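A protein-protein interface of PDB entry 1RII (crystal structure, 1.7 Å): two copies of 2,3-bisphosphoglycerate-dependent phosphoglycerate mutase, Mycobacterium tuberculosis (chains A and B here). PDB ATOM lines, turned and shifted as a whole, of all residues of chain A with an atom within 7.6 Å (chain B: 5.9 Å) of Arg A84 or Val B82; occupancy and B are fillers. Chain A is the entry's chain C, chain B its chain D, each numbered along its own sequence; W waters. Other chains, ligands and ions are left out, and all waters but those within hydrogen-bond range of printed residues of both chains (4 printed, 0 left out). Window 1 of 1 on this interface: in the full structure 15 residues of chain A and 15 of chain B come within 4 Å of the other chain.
Water W2 lies within hydrogen-bond range of O of Leu B78, O of Ile B80 and NH2 of Arg A84. Water W4 lies within hydrogen-bond range of the backbone carbonyl oxygen of Val A82 (2.7 Å), the backbone NH of Val B82 (2.9 Å) and the guanidinium group of Arg B83 (3.0 Å). Water W3 lies within hydrogen-bond range of O of Val B82 (2.7 Å), N of Val A82 (2.8 Å) and NH1 of Arg A83 (3.1 Å). Water W1 bridges a ring nitrogen (ND1) of His A69 and the guanidinium group of Arg B84.
O of Leu B78 sits at hydrogen-bond distance from NE of Arg A84 (3.4 Å). The backbone carbonyl oxygen (O) of Ile A80 is in hydrogen-bond range of the guanidinium group (NH1) of Arg B84 (2.6 Å). The guanidinium group (NH1) of Arg B84 lies within hydrogen-bond range of the backbone carbonyl oxygen (O) of Leu A78.
Among the printed residues, merely in contact across the chains: Val A82 with Arg B84 (3.2 Å), Leu A60 with Trp B79 (3.5 Å), Arg A84 with Trp B79 (3.5 Å), Arg A83 with Arg B83 (3.5 Å), Arg A84 with Ile B80 (3.6 Å), Val A82 with Val B82 (3.7 Å), Ile A65 with Leu B78 (3.9 Å), Ile A65 with Trp B79 (3.9 Å), Arg A84 with Val B82 (3.9 Å) and Val A82 with Arg B83 (3.97 Å).
Of the 23 printed residues of chain A, 7 touch a printed residue of chain B. Hydrophobic or aromatic side chains of chain A that line the printed part of chain B: Leu A60, Ile A65 and Val A82. Hydrophobic or aromatic side chains of chain B that line the printed part of chain A: Leu B78, Trp B79 and Val B82. Among the printed residues, 13 pairs touch across the chains.
Ile A80 touches Arg B84, and with the chains exchanged Arg A84 touches Ile B80. Val A82 touches its own counterpart, Val B82. Val A82 touches Arg B83, but with the chains exchanged Arg A83 does not touch Val B82 (4.3 Å). Arg A83 touches its own counterpart, Arg B83. 9 positions are printed for both chains.
OG1 of Thr A58 is in hydrogen-bond range of NH1 of Arg A84 (3.1 Å). The backbone NH of Leu A60 sits at hydrogen-bond distance from the side-chain amide oxygen of Asn A89 (3.0 Å). N of Thr A58 is in hydrogen-bond range of O of Arg A83 (3.1 Å). The backbone carbonyl oxygen of Leu B56 is in hydrogen-bond range of the backbone NH of Arg B83. The backbone NH (N) of Arg A83 lies within hydrogen-bond range of the backbone carbonyl oxygen (O) of Leu A56. N of Thr B58 sits at hydrogen-bond distance from O of Arg B83.
Of the printed residues of chain B, Leu A60 touches Trp B79. Printed residues of chain B within 4 Å of Ile A65: Leu B78 (3.9 Å) and Trp B79 (3.9 Å). Of the printed residues of chain B, Val A82 touches Val B82, Arg B83 and Arg B84. Of chain B, only Leu B78 (3.4 Å), Trp B79 (3.5 Å), Ile B80 (3.6 Å) and Val B82 (3.9 Å) come within 4 Å of Arg A84. Ser A85 touches none of the printed residues of chain B. Printed residues of chain A within 4 Å of Trp B79: Leu A60, Ile A65 and Arg A84. Val B82 touches just these residues of chain A: Val A82 and Arg A84. Printed residues of chain A within 4 Å of Arg B83: Val A82 (3.97 Å) and Arg A83 (3.5 Å). The nearest printed residue of chain B that does not touch Arg A84 is Arg B84 (5.2 Å). The nearest residue of chain A that does not touch Val B82 is Arg A83 (4.3 Å).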
ATOM      1  N   LEU A  56      19.841   6.769  -9.135  1.00  0.00           N
ATOM      2  CA  LEU A  56      18.738   6.906  -8.208  1.00  0.00           C
ATOM      3  C   LEU A  56      17.687   7.880  -8.740  1.00  0.00           C
ATOM      4  O   LEU A  56      18.053   8.955  -9.208  1.00  0.00           O
ATOM      5  CB  LEU A  56      19.233   7.410  -6.861  1.00  0.00           C
ATOM      6  CG  LEU A  56      18.173   7.966  -5.907  1.00  0.00           C
ATOM      7  CD1 LEU A  56      17.286   6.828  -5.430  1.00  0.00           C
ATOM      8  CD2 LEU A  56      18.826   8.714  -4.763  1.00  0.00           C
ATOM      9  N   TYR A  57      16.433   7.469  -8.629  1.00  0.00           N
ATOM     10  CA  TYR A  57      15.277   8.301  -8.930  1.00  0.00           C
ATOM     11  C   TYR A  57      14.404   8.446  -7.695  1.00  0.00           C
ATOM     12  O   TYR A  57      14.066   7.424  -7.080  1.00  0.00           O
ATOM     13  CB  TYR A  57      14.449   7.730 -10.085  1.00  0.00           C
ATOM     14  CG  TYR A  57      15.152   7.830 -11.428  1.00  0.00           C
ATOM     15  CD1 TYR A  57      15.166   9.022 -12.144  1.00  0.00           C
ATOM     16  CD2 TYR A  57      15.801   6.741 -11.996  1.00  0.00           C
ATOM     17  CE1 TYR A  57      15.803   9.110 -13.369  1.00  0.00           C
ATOM     18  CE2 TYR A  57      16.442   6.823 -13.213  1.00  0.00           C
ATOM     19  CZ  TYR A  57      16.443   8.007 -13.912  1.00  0.00           C
ATOM     20  OH  TYR A  57      17.084   8.124 -15.120  1.00  0.00           O
ATOM     21  N   THR A  58      14.044   9.666  -7.325  1.00  0.00           N
ATOM     22  CA  THR A  58      13.141   9.868  -6.192  1.00  0.00           C
ATOM     23  C   THR A  58      12.036  10.860  -6.550  1.00  0.00           C
ATOM     24  O   THR A  58      12.041  11.463  -7.624  1.00  0.00           O
ATOM     25  CB  THR A  58      13.825  10.429  -4.926  1.00  0.00           C
ATOM     26  OG1 THR A  58      14.173  11.790  -5.216  1.00  0.00           O
ATOM     27  CG2 THR A  58      15.125   9.735  -4.555  1.00  0.00           C
ATOM     28  N   SER A  59      11.095  11.055  -5.622  1.00  0.00           N
ATOM     29  CA  SER A  59      10.088  12.096  -5.738  1.00  0.00           C
ATOM     30  C   SER A  59      10.667  13.413  -5.220  1.00  0.00           C
ATOM     31  O   SER A  59      11.865  13.511  -4.921  1.00  0.00           O
ATOM     32  CB  SER A  59       8.830  11.703  -4.958  1.00  0.00           C
ATOM     33  OG  SER A  59       9.103  11.662  -3.575  1.00  0.00           O
ATOM     34  N   LEU A  60       9.853  14.450  -5.056  1.00  0.00           N
ATOM     35  CA  LEU A  60      10.373  15.674  -4.437  1.00  0.00           C
ATOM     36  C   LEU A  60      10.092  15.703  -2.939  1.00  0.00           C
ATOM     37  O   LEU A  60      10.290  16.733  -2.303  1.00  0.00           O
ATOM     38  CB  LEU A  60       9.777  16.890  -5.139  1.00  0.00           C
ATOM     39  CG  LEU A  60       9.971  16.927  -6.667  1.00  0.00           C
ATOM     40  CD1 LEU A  60       9.242  18.117  -7.259  1.00  0.00           C
ATOM     41  CD2 LEU A  60      11.448  16.930  -7.032  1.00  0.00           C
ATOM     42  N   LEU A  61       9.624  14.594  -2.373  1.00  0.00           N
ATOM     43  CA  LEU A  61       9.196  14.560  -0.984  1.00  0.00           C
ATOM     44  C   LEU A  61      10.292  13.989  -0.089  1.00  0.00           C
ATOM     45  O   LEU A  61      10.804  12.933  -0.420  1.00  0.00           O
ATOM     46  CB  LEU A  61       7.897  13.759  -0.829  1.00  0.00           C
ATOM     47  CG  LEU A  61       6.751  14.256  -1.734  1.00  0.00           C
ATOM     48  CD1 LEU A  61       5.518  13.374  -1.612  1.00  0.00           C
ATOM     49  CD2 LEU A  61       6.375  15.699  -1.426  1.00  0.00           C
ATOM     50  N   ALA A  64      10.903  10.271   1.048  1.00  0.00           N
ATOM     51  CA  ALA A  64      11.460   9.444  -0.010  1.00  0.00           C
ATOM     52  C   ALA A  64      12.951   9.741  -0.182  1.00  0.00           C
ATOM     53  O   ALA A  64      13.804   8.862  -0.237  1.00  0.00           O
ATOM     54  CB  ALA A  64      10.737   9.661  -1.349  1.00  0.00           C
ATOM     55  N   ILE A  65      13.255  11.031  -0.275  1.00  0.00           N
ATOM     56  CA  ILE A  65      14.660  11.413  -0.497  1.00  0.00           C
ATOM     57  C   ILE A  65      15.538  10.955   0.644  1.00  0.00           C
ATOM     58  O   ILE A  65      16.636  10.416   0.464  1.00  0.00           O
ATOM     59  CB  ILE A  65      14.718  12.939  -0.685  1.00  0.00           C
ATOM     60  CG1 ILE A  65      13.899  13.364  -1.917  1.00  0.00           C
ATOM     61  CG2 ILE A  65      16.138  13.449  -0.723  1.00  0.00           C
ATOM     62  CD1 ILE A  65      13.597  14.844  -1.950  1.00  0.00           C
ATOM     63  N   THR A  66      15.081  11.153   1.877  1.00  0.00           N
ATOM     64  CA  THR A  66      15.863  10.699   3.026  1.00  0.00           C
ATOM     65  C   THR A  66      15.949   9.183   3.091  1.00  0.00           C
ATOM     66  O   THR A  66      16.982   8.604   3.450  1.00  0.00           O
ATOM     67  CB  THR A  66      15.246  11.243   4.324  1.00  0.00           C
ATOM     68  OG1 THR A  66      15.430  12.662   4.338  1.00  0.00           O
ATOM     69  CG2 THR A  66      15.953  10.679   5.545  1.00  0.00           C
ATOM     70  N   ALA A  68      16.042   7.260   0.539  1.00  0.00           N
ATOM     71  CA  ALA A  68      17.042   6.970  -0.485  1.00  0.00           C
ATOM     72  C   ALA A  68      18.456   7.218   0.012  1.00  0.00           C
ATOM     73  O   ALA A  68      19.352   6.404  -0.192  1.00  0.00           O
ATOM     74  CB  ALA A  68      16.788   7.804  -1.733  1.00  0.00           C
ATOM     75  N   HIS A  69      18.650   8.355   0.685  1.00  0.00           N
ATOM     76  CA  HIS A  69      19.968   8.653   1.220  1.00  0.00           C
ATOM     77  C   HIS A  69      20.471   7.601   2.204  1.00  0.00           C
ATOM     78  O   HIS A  69      21.628   7.188   2.161  1.00  0.00           O
ATOM     79  CB  HIS A  69      19.920  10.021   1.923  1.00  0.00           C
ATOM     80  CG  HIS A  69      21.158  10.307   2.717  1.00  0.00           C
ATOM     81  ND1 HIS A  69      22.283  10.846   2.126  1.00  0.00           N
ATOM     82  CD2 HIS A  69      21.463  10.159   4.022  1.00  0.00           C
ATOM     83  CE1 HIS A  69      23.220  11.004   3.039  1.00  0.00           C
ATOM     84  NE2 HIS A  69      22.754  10.590   4.198  1.00  0.00           N
ATOM     85  N   LEU A  78      26.319   6.052  -2.108  1.00  0.00           N
ATOM     86  CA  LEU A  78      25.920   7.435  -1.908  1.00  0.00           C
ATOM     87  C   LEU A  78      26.321   8.316  -3.085  1.00  0.00           C
ATOM     88  O   LEU A  78      25.737   9.394  -3.263  1.00  0.00           O
ATOM     89  CB  LEU A  78      26.593   8.054  -0.679  1.00  0.00           C
ATOM     90  CG  LEU A  78      25.852   8.645   0.498  1.00  0.00           C
ATOM     91  CD1 LEU A  78      24.364   8.337   0.462  1.00  0.00           C
ATOM     92  CD2 LEU A  78      26.507   8.171   1.794  1.00  0.00           C
ATOM     93  N   ILE A  80      26.278   7.912  -6.291  1.00  0.00           N
ATOM     94  CA  ILE A  80      25.742   7.716  -7.637  1.00  0.00           C
ATOM     95  C   ILE A  80      24.858   8.880  -8.040  1.00  0.00           C
ATOM     96  O   ILE A  80      24.355   9.623  -7.206  1.00  0.00           O
ATOM     97  CB  ILE A  80      24.963   6.397  -7.737  1.00  0.00           C
ATOM     98  CG1 ILE A  80      23.679   6.374  -6.898  1.00  0.00           C
ATOM     99  CG2 ILE A  80      25.880   5.221  -7.400  1.00  0.00           C
ATOM    100  CD1 ILE A  80      22.881   5.095  -7.115  1.00  0.00           C
ATOM    101  N   PRO A  81      24.674   9.065  -9.328  1.00  0.00           N
ATOM    102  CA  PRO A  81      23.814  10.144  -9.788  1.00  0.00           C
ATOM    103  C   PRO A  81      22.360   9.956  -9.365  1.00  0.00           C
ATOM    104  O   PRO A  81      21.867   8.840  -9.224  1.00  0.00           O
ATOM    105  CB  PRO A  81      23.860  10.019 -11.307  1.00  0.00           C
ATOM    106  CG  PRO A  81      25.062   9.213 -11.620  1.00  0.00           C
ATOM    107  CD  PRO A  81      25.252   8.297 -10.451  1.00  0.00           C
ATOM    108  N   VAL A  82      21.711  11.103  -9.187  1.00  0.00           N
ATOM    109  CA  VAL A  82      20.324  11.130  -8.761  1.00  0.00           C
ATOM    110  C   VAL A  82      19.525  12.170  -9.538  1.00  0.00           C
ATOM    111  O   VAL A  82      19.983  13.255  -9.916  1.00  0.00           O
ATOM    112  CB  VAL A  82      20.212  11.399  -7.244  1.00  0.00           C
ATOM    113  CG1 VAL A  82      21.525  11.908  -6.682  1.00  0.00           C
ATOM    114  CG2 VAL A  82      19.087  12.369  -6.921  1.00  0.00           C
ATOM    115  N   ARG A  83      18.280  11.773  -9.775  1.00  0.00           N
ATOM    116  CA  ARG A  83      17.336  12.636 -10.466  1.00  0.00           C
ATOM    117  C   ARG A  83      16.014  12.596  -9.716  1.00  0.00           C
ATOM    118  O   ARG A  83      15.657  11.504  -9.257  1.00  0.00           O
ATOM    119  CB  ARG A  83      17.157  12.168 -11.918  1.00  0.00           C
ATOM    120  CG  ARG A  83      18.462  12.214 -12.698  1.00  0.00           C
ATOM    121  CD  ARG A  83      18.789  13.648 -13.078  1.00  0.00           C
ATOM    122  NE  ARG A  83      19.946  13.717 -13.955  1.00  0.00           N
ATOM    123  CZ  ARG A  83      21.212  13.566 -13.596  1.00  0.00           C
ATOM    124  NH1 ARG A  83      21.566  13.324 -12.341  1.00  0.00           N
ATOM    125  NH2 ARG A  83      22.170  13.659 -14.523  1.00  0.00           N
ATOM    126  N   ARG A  84      15.356  13.735  -9.593  1.00  0.00           N
ATOM    127  CA  ARG A  84      14.120  13.831  -8.820  1.00  0.00           C
ATOM    128  C   ARG A  84      13.040  14.469  -9.689  1.00  0.00           C
ATOM    129  O   ARG A  84      13.313  15.302 -10.547  1.00  0.00           O
ATOM    130  CB  ARG A  84      14.314  14.599  -7.533  1.00  0.00           C
ATOM    131  CG  ARG A  84      15.618  14.359  -6.780  1.00  0.00           C
ATOM    132  CD  ARG A  84      15.581  15.146  -5.471  1.00  0.00           C
ATOM    133  NE  ARG A  84      16.825  15.200  -4.714  1.00  0.00           N
ATOM    134  CZ  ARG A  84      17.419  14.170  -4.134  1.00  0.00           C
ATOM    135  NH1 ARG A  84      16.868  12.969  -4.231  1.00  0.00           N
ATOM    136  NH2 ARG A  84      18.555  14.340  -3.467  1.00  0.00           N
ATOM    137  N   SER A  85      11.801  14.016  -9.466  1.00  0.00           N
ATOM    138  CA  SER A  85      10.672  14.494 -10.246  1.00  0.00           C
ATOM    139  C   SER A  85       9.386  14.407  -9.425  1.00  0.00           C
ATOM    140  O   SER A  85       9.097  13.457  -8.695  1.00  0.00           O
ATOM    141  CB  SER A  85      10.520  13.697 -11.544  1.00  0.00           C
ATOM    142  OG  SER A  85       9.310  13.961 -12.228  1.00  0.00           O
ATOM    143  N   TRP A  86       8.570  15.443  -9.592  1.00  0.00           N
ATOM    144  CA  TRP A  86       7.230  15.448  -9.041  1.00  0.00           C
ATOM    145  C   TRP A  86       6.444  14.242  -9.550  1.00  0.00           C
ATOM    146  O   TRP A  86       5.502  13.786  -8.890  1.00  0.00           O
ATOM    147  CB  TRP A  86       6.532  16.767  -9.392  1.00  0.00           C
ATOM    148  CG  TRP A  86       6.001  16.872 -10.783  1.00  0.00           C
ATOM    149  CD1 TRP A  86       6.643  17.344 -11.888  1.00  0.00           C
ATOM    150  CD2 TRP A  86       4.688  16.494 -11.230  1.00  0.00           C
ATOM    151  NE1 TRP A  86       5.825  17.282 -12.993  1.00  0.00           N
ATOM    152  CE2 TRP A  86       4.615  16.766 -12.613  1.00  0.00           C
ATOM    153  CE3 TRP A  86       3.568  15.955 -10.601  1.00  0.00           C
ATOM    154  CZ2 TRP A  86       3.473  16.516 -13.368  1.00  0.00           C
ATOM    155  CZ3 TRP A  86       2.432  15.706 -11.352  1.00  0.00           C
ATOM    156  CH2 TRP A  86       2.383  15.985 -12.728  1.00  0.00           C
ATOM    157  N   ARG A  87       6.789  13.694 -10.710  1.00  0.00           N
ATOM    158  CA  ARG A  87       6.007  12.595 -11.273  1.00  0.00           C
ATOM    159  C   ARG A  87       6.147  11.317 -10.459  1.00  0.00           C
ATOM    160  O   ARG A  87       5.352  10.392 -10.665  1.00  0.00           O
ATOM    161  CB  ARG A  87       6.385  12.387 -12.744  1.00  0.00           C
ATOM    162  CG  ARG A  87       6.116  13.641 -13.574  1.00  0.00           C
ATOM    163  CD  ARG A  87       6.397  13.438 -15.054  1.00  0.00           C
ATOM    164  NE  ARG A  87       6.008  14.649 -15.776  1.00  0.00           N
ATOM    165  CZ  ARG A  87       4.831  14.889 -16.330  1.00  0.00           C
ATOM    166  NH1 ARG A  87       3.868  13.986 -16.267  1.00  0.00           N
ATOM    167  NH2 ARG A  87       4.604  16.047 -16.958  1.00  0.00           N
ATOM    168  N   LEU A  88       7.119  11.281  -9.535  1.00  0.00           N
ATOM    169  CA  LEU A  88       7.215  10.146  -8.621  1.00  0.00           C
ATOM    170  C   LEU A  88       6.545  10.447  -7.292  1.00  0.00           C
ATOM    171  O   LEU A  88       6.578   9.612  -6.387  1.00  0.00           O
ATOM    172  CB  LEU A  88       8.678   9.733  -8.391  1.00  0.00           C
ATOM    173  CG  LEU A  88       9.283   8.827  -9.472  1.00  0.00           C
ATOM    174  CD1 LEU A  88       9.126   9.481 -10.839  1.00  0.00           C
ATOM    175  CD2 LEU A  88      10.747   8.525  -9.238  1.00  0.00           C
ATOM    176  N   ASN A  89       5.933  11.610  -7.121  1.00  0.00           N
ATOM    177  CA  ASN A  89       5.311  11.973  -5.858  1.00  0.00           C
ATOM    178  C   ASN A  89       4.176  11.010  -5.508  1.00  0.00           C
ATOM    179  O   ASN A  89       3.581  10.393  -6.380  1.00  0.00           O
ATOM    180  CB  ASN A  89       4.720  13.386  -5.886  1.00  0.00           C
ATOM    181  CG  ASN A  89       5.687  14.506  -5.611  1.00  0.00           C
ATOM    182  OD1 ASN A  89       6.908  14.337  -5.601  1.00  0.00           O
ATOM    183  ND2 ASN A  89       5.174  15.719  -5.373  1.00  0.00           N
ATOM    184  N   TYR A 163       7.381   9.917 -17.446  1.00  0.00           N
ATOM    185  CA  TYR A 163       8.694   9.941 -16.812  1.00  0.00           C
ATOM    186  C   TYR A 163       9.383   8.589 -16.891  1.00  0.00           C
ATOM    187  O   TYR A 163      10.568   8.380 -17.168  1.00  0.00           O
ATOM    188  CB  TYR A 163       8.576  10.380 -15.343  1.00  0.00           C
ATOM    189  CG  TYR A 163       9.952  10.737 -14.806  1.00  0.00           C
ATOM    190  CD1 TYR A 163      10.556  11.934 -15.168  1.00  0.00           C
ATOM    191  CD2 TYR A 163      10.645   9.897 -13.950  1.00  0.00           C
ATOM    192  CE1 TYR A 163      11.808  12.269 -14.680  1.00  0.00           C
ATOM    193  CE2 TYR A 163      11.898  10.217 -13.460  1.00  0.00           C
ATOM    194  CZ  TYR A 163      12.477  11.412 -13.832  1.00  0.00           C
ATOM    195  OH  TYR A 163      13.725  11.759 -13.368  1.00  0.00           O
ATOM    196  N   VAL B  55      20.449  24.632  -6.789  1.00  0.00           N
ATOM    197  CA  VAL B  55      21.169  23.423  -7.173  1.00  0.00           C
ATOM    198  C   VAL B  55      22.330  23.158  -6.211  1.00  0.00           C
ATOM    199  O   VAL B  55      22.866  24.099  -5.622  1.00  0.00           O
ATOM    200  CB  VAL B  55      21.720  23.508  -8.610  1.00  0.00           C
ATOM    201  CG1 VAL B  55      22.698  24.665  -8.704  1.00  0.00           C
ATOM    202  CG2 VAL B  55      22.360  22.194  -9.029  1.00  0.00           C
ATOM    203  N   LEU B  56      22.673  21.885  -6.073  1.00  0.00           N
ATOM    204  CA  LEU B  56      23.721  21.405  -5.190  1.00  0.00           C
ATOM    205  C   LEU B  56      24.799  20.678  -5.972  1.00  0.00           C
ATOM    206  O   LEU B  56      24.483  19.801  -6.775  1.00  0.00           O
ATOM    207  CB  LEU B  56      23.163  20.461  -4.119  1.00  0.00           C
ATOM    208  CG  LEU B  56      24.197  19.603  -3.380  1.00  0.00           C
ATOM    209  CD1 LEU B  56      25.011  20.439  -2.406  1.00  0.00           C
ATOM    210  CD2 LEU B  56      23.531  18.455  -2.635  1.00  0.00           C
ATOM    211  N   TYR B  57      26.052  21.040  -5.713  1.00  0.00           N
ATOM    212  CA  TYR B  57      27.151  20.234  -6.236  1.00  0.00           C
ATOM    213  C   TYR B  57      27.957  19.623  -5.095  1.00  0.00           C
ATOM    214  O   TYR B  57      28.281  20.306  -4.114  1.00  0.00           O
ATOM    215  CB  TYR B  57      28.039  21.109  -7.134  1.00  0.00           C
ATOM    216  CG  TYR B  57      27.309  21.552  -8.394  1.00  0.00           C
ATOM    217  CD1 TYR B  57      27.296  20.715  -9.505  1.00  0.00           C
ATOM    218  CD2 TYR B  57      26.651  22.764  -8.497  1.00  0.00           C
ATOM    219  CE1 TYR B  57      26.648  21.088 -10.659  1.00  0.00           C
ATOM    220  CE2 TYR B  57      25.989  23.153  -9.649  1.00  0.00           C
ATOM    221  CZ  TYR B  57      25.997  22.301 -10.738  1.00  0.00           C
ATOM    222  OH  TYR B  57      25.354  22.616 -11.919  1.00  0.00           O
ATOM    223  N   THR B  58      28.291  18.336  -5.179  1.00  0.00           N
ATOM    224  CA  THR B  58      29.135  17.732  -4.163  1.00  0.00           C
ATOM    225  C   THR B  58      30.246  16.901  -4.812  1.00  0.00           C
ATOM    226  O   THR B  58      30.250  16.668  -6.009  1.00  0.00           O
ATOM    227  CB  THR B  58      28.399  16.782  -3.201  1.00  0.00           C
ATOM    228  OG1 THR B  58      28.068  15.583  -3.930  1.00  0.00           O
ATOM    229  CG2 THR B  58      27.115  17.398  -2.689  1.00  0.00           C
ATOM    230  N   LEU B  78      15.697  20.087   0.161  1.00  0.00           N
ATOM    231  CA  LEU B  78      16.121  18.725  -0.155  1.00  0.00           C
ATOM    232  C   LEU B  78      15.794  18.302  -1.579  1.00  0.00           C
ATOM    233  O   LEU B  78      16.476  17.447  -2.152  1.00  0.00           O
ATOM    234  CB  LEU B  78      15.467  17.705   0.779  1.00  0.00           C
ATOM    235  CG  LEU B  78      16.265  16.655   1.518  1.00  0.00           C
ATOM    236  CD1 LEU B  78      17.739  16.980   1.702  1.00  0.00           C
ATOM    237  CD2 LEU B  78      15.619  16.397   2.888  1.00  0.00           C
ATOM    238  N   TRP B  79      14.742  18.861  -2.148  1.00  0.00           N
ATOM    239  CA  TRP B  79      14.192  18.408  -3.415  1.00  0.00           C
ATOM    240  C   TRP B  79      14.982  18.896  -4.614  1.00  0.00           C
ATOM    241  O   TRP B  79      14.710  18.542  -5.757  1.00  0.00           O
ATOM    242  CB  TRP B  79      12.747  18.916  -3.544  1.00  0.00           C
ATOM    243  CG  TRP B  79      12.643  20.398  -3.329  1.00  0.00           C
ATOM    244  CD1 TRP B  79      12.400  21.031  -2.149  1.00  0.00           C
ATOM    245  CD2 TRP B  79      12.777  21.434  -4.297  1.00  0.00           C
ATOM    246  NE1 TRP B  79      12.371  22.394  -2.311  1.00  0.00           N
ATOM    247  CE2 TRP B  79      12.602  22.665  -3.633  1.00  0.00           C
ATOM    248  CE3 TRP B  79      13.030  21.432  -5.664  1.00  0.00           C
ATOM    249  CZ2 TRP B  79      12.669  23.888  -4.291  1.00  0.00           C
ATOM    250  CZ3 TRP B  79      13.101  22.639  -6.326  1.00  0.00           C
ATOM    251  CH2 TRP B  79      12.922  23.842  -5.637  1.00  0.00           C
ATOM    252  N   ILE B  80      15.970  19.764  -4.411  1.00  0.00           N
ATOM    253  CA  ILE B  80      16.608  20.408  -5.547  1.00  0.00           C
ATOM    254  C   ILE B  80      17.550  19.463  -6.277  1.00  0.00           C
ATOM    255  O   ILE B  80      17.994  18.483  -5.671  1.00  0.00           O
ATOM    256  CB  ILE B  80      17.434  21.639  -5.124  1.00  0.00           C
ATOM    257  CG1 ILE B  80      18.614  21.268  -4.210  1.00  0.00           C
ATOM    258  CG2 ILE B  80      16.510  22.674  -4.521  1.00  0.00           C
ATOM    259  CD1 ILE B  80      19.398  22.443  -3.674  1.00  0.00           C
ATOM    260  N   PRO B  81      17.846  19.774  -7.531  1.00  0.00           N
ATOM    261  CA  PRO B  81      18.775  18.954  -8.304  1.00  0.00           C
ATOM    262  C   PRO B  81      20.153  18.929  -7.654  1.00  0.00           C
ATOM    263  O   PRO B  81      20.561  19.930  -7.080  1.00  0.00           O
ATOM    264  CB  PRO B  81      18.903  19.684  -9.642  1.00  0.00           C
ATOM    265  CG  PRO B  81      17.612  20.430  -9.748  1.00  0.00           C
ATOM    266  CD  PRO B  81      17.340  20.904  -8.340  1.00  0.00           C
ATOM    267  N   VAL B  82      20.790  17.786  -7.795  1.00  0.00           N
ATOM    268  CA  VAL B  82      22.123  17.523  -7.284  1.00  0.00           C
ATOM    269  C   VAL B  82      22.966  16.851  -8.349  1.00  0.00           C
ATOM    270  O   VAL B  82      22.532  15.941  -9.070  1.00  0.00           O
ATOM    271  CB  VAL B  82      22.088  16.640  -6.025  1.00  0.00           C
ATOM    272  CG1 VAL B  82      21.100  15.508  -6.193  1.00  0.00           C
ATOM    273  CG2 VAL B  82      23.503  16.120  -5.743  1.00  0.00           C
ATOM    274  N   ARG B  83      24.216  17.334  -8.430  1.00  0.00           N
ATOM    275  CA  ARG B  83      25.181  16.681  -9.303  1.00  0.00           C
ATOM    276  C   ARG B  83      26.464  16.435  -8.528  1.00  0.00           C
ATOM    277  O   ARG B  83      26.797  17.260  -7.668  1.00  0.00           O
ATOM    278  CB  ARG B  83      25.493  17.568 -10.515  1.00  0.00           C
ATOM    279  CG  ARG B  83      24.273  17.890 -11.363  1.00  0.00           C
ATOM    280  CD  ARG B  83      23.925  16.724 -12.274  1.00  0.00           C
ATOM    281  NE  ARG B  83      22.732  16.950 -13.065  1.00  0.00           N
ATOM    282  CZ  ARG B  83      21.467  16.961 -12.694  1.00  0.00           C
ATOM    283  NH1 ARG B  83      21.105  16.745 -11.444  1.00  0.00           N
ATOM    284  NH2 ARG B  83      20.529  17.197 -13.618  1.00  0.00           N
ATOM    285  N   ARG B  84      27.131  15.318  -8.792  1.00  0.00           N
ATOM    286  CA  ARG B  84      28.342  14.970  -8.063  1.00  0.00           C
ATOM    287  C   ARG B  84      29.507  14.747  -9.023  1.00  0.00           C
ATOM    288  O   ARG B  84      29.350  14.289 -10.161  1.00  0.00           O
ATOM    289  CB  ARG B  84      28.063  13.755  -7.176  1.00  0.00           C
ATOM    290  CG  ARG B  84      26.773  13.883  -6.359  1.00  0.00           C
ATOM    291  CD  ARG B  84      26.558  12.617  -5.538  1.00  0.00           C
ATOM    292  NE  ARG B  84      25.375  12.624  -4.743  1.00  0.00           N
ATOM    293  CZ  ARG B  84      24.296  12.013  -4.402  1.00  0.00           C
ATOM    294  NH1 ARG B  84      23.960  10.823  -4.911  1.00  0.00           N
ATOM    295  NH2 ARG B  84      23.468  12.570  -3.500  1.00  0.00           N
HETATM  296  O   HOH W   1      22.209  12.211  -0.335  1.00  0.00           O
HETATM  297  O   HOH W   2      18.827  17.311  -3.281  1.00  0.00           O
HETATM  298  O   HOH W   3      23.255  13.413  -9.794  1.00  0.00           O
HETATM  299  O   HOH W   4      19.330  15.780  -9.201  1.00  0.00           O
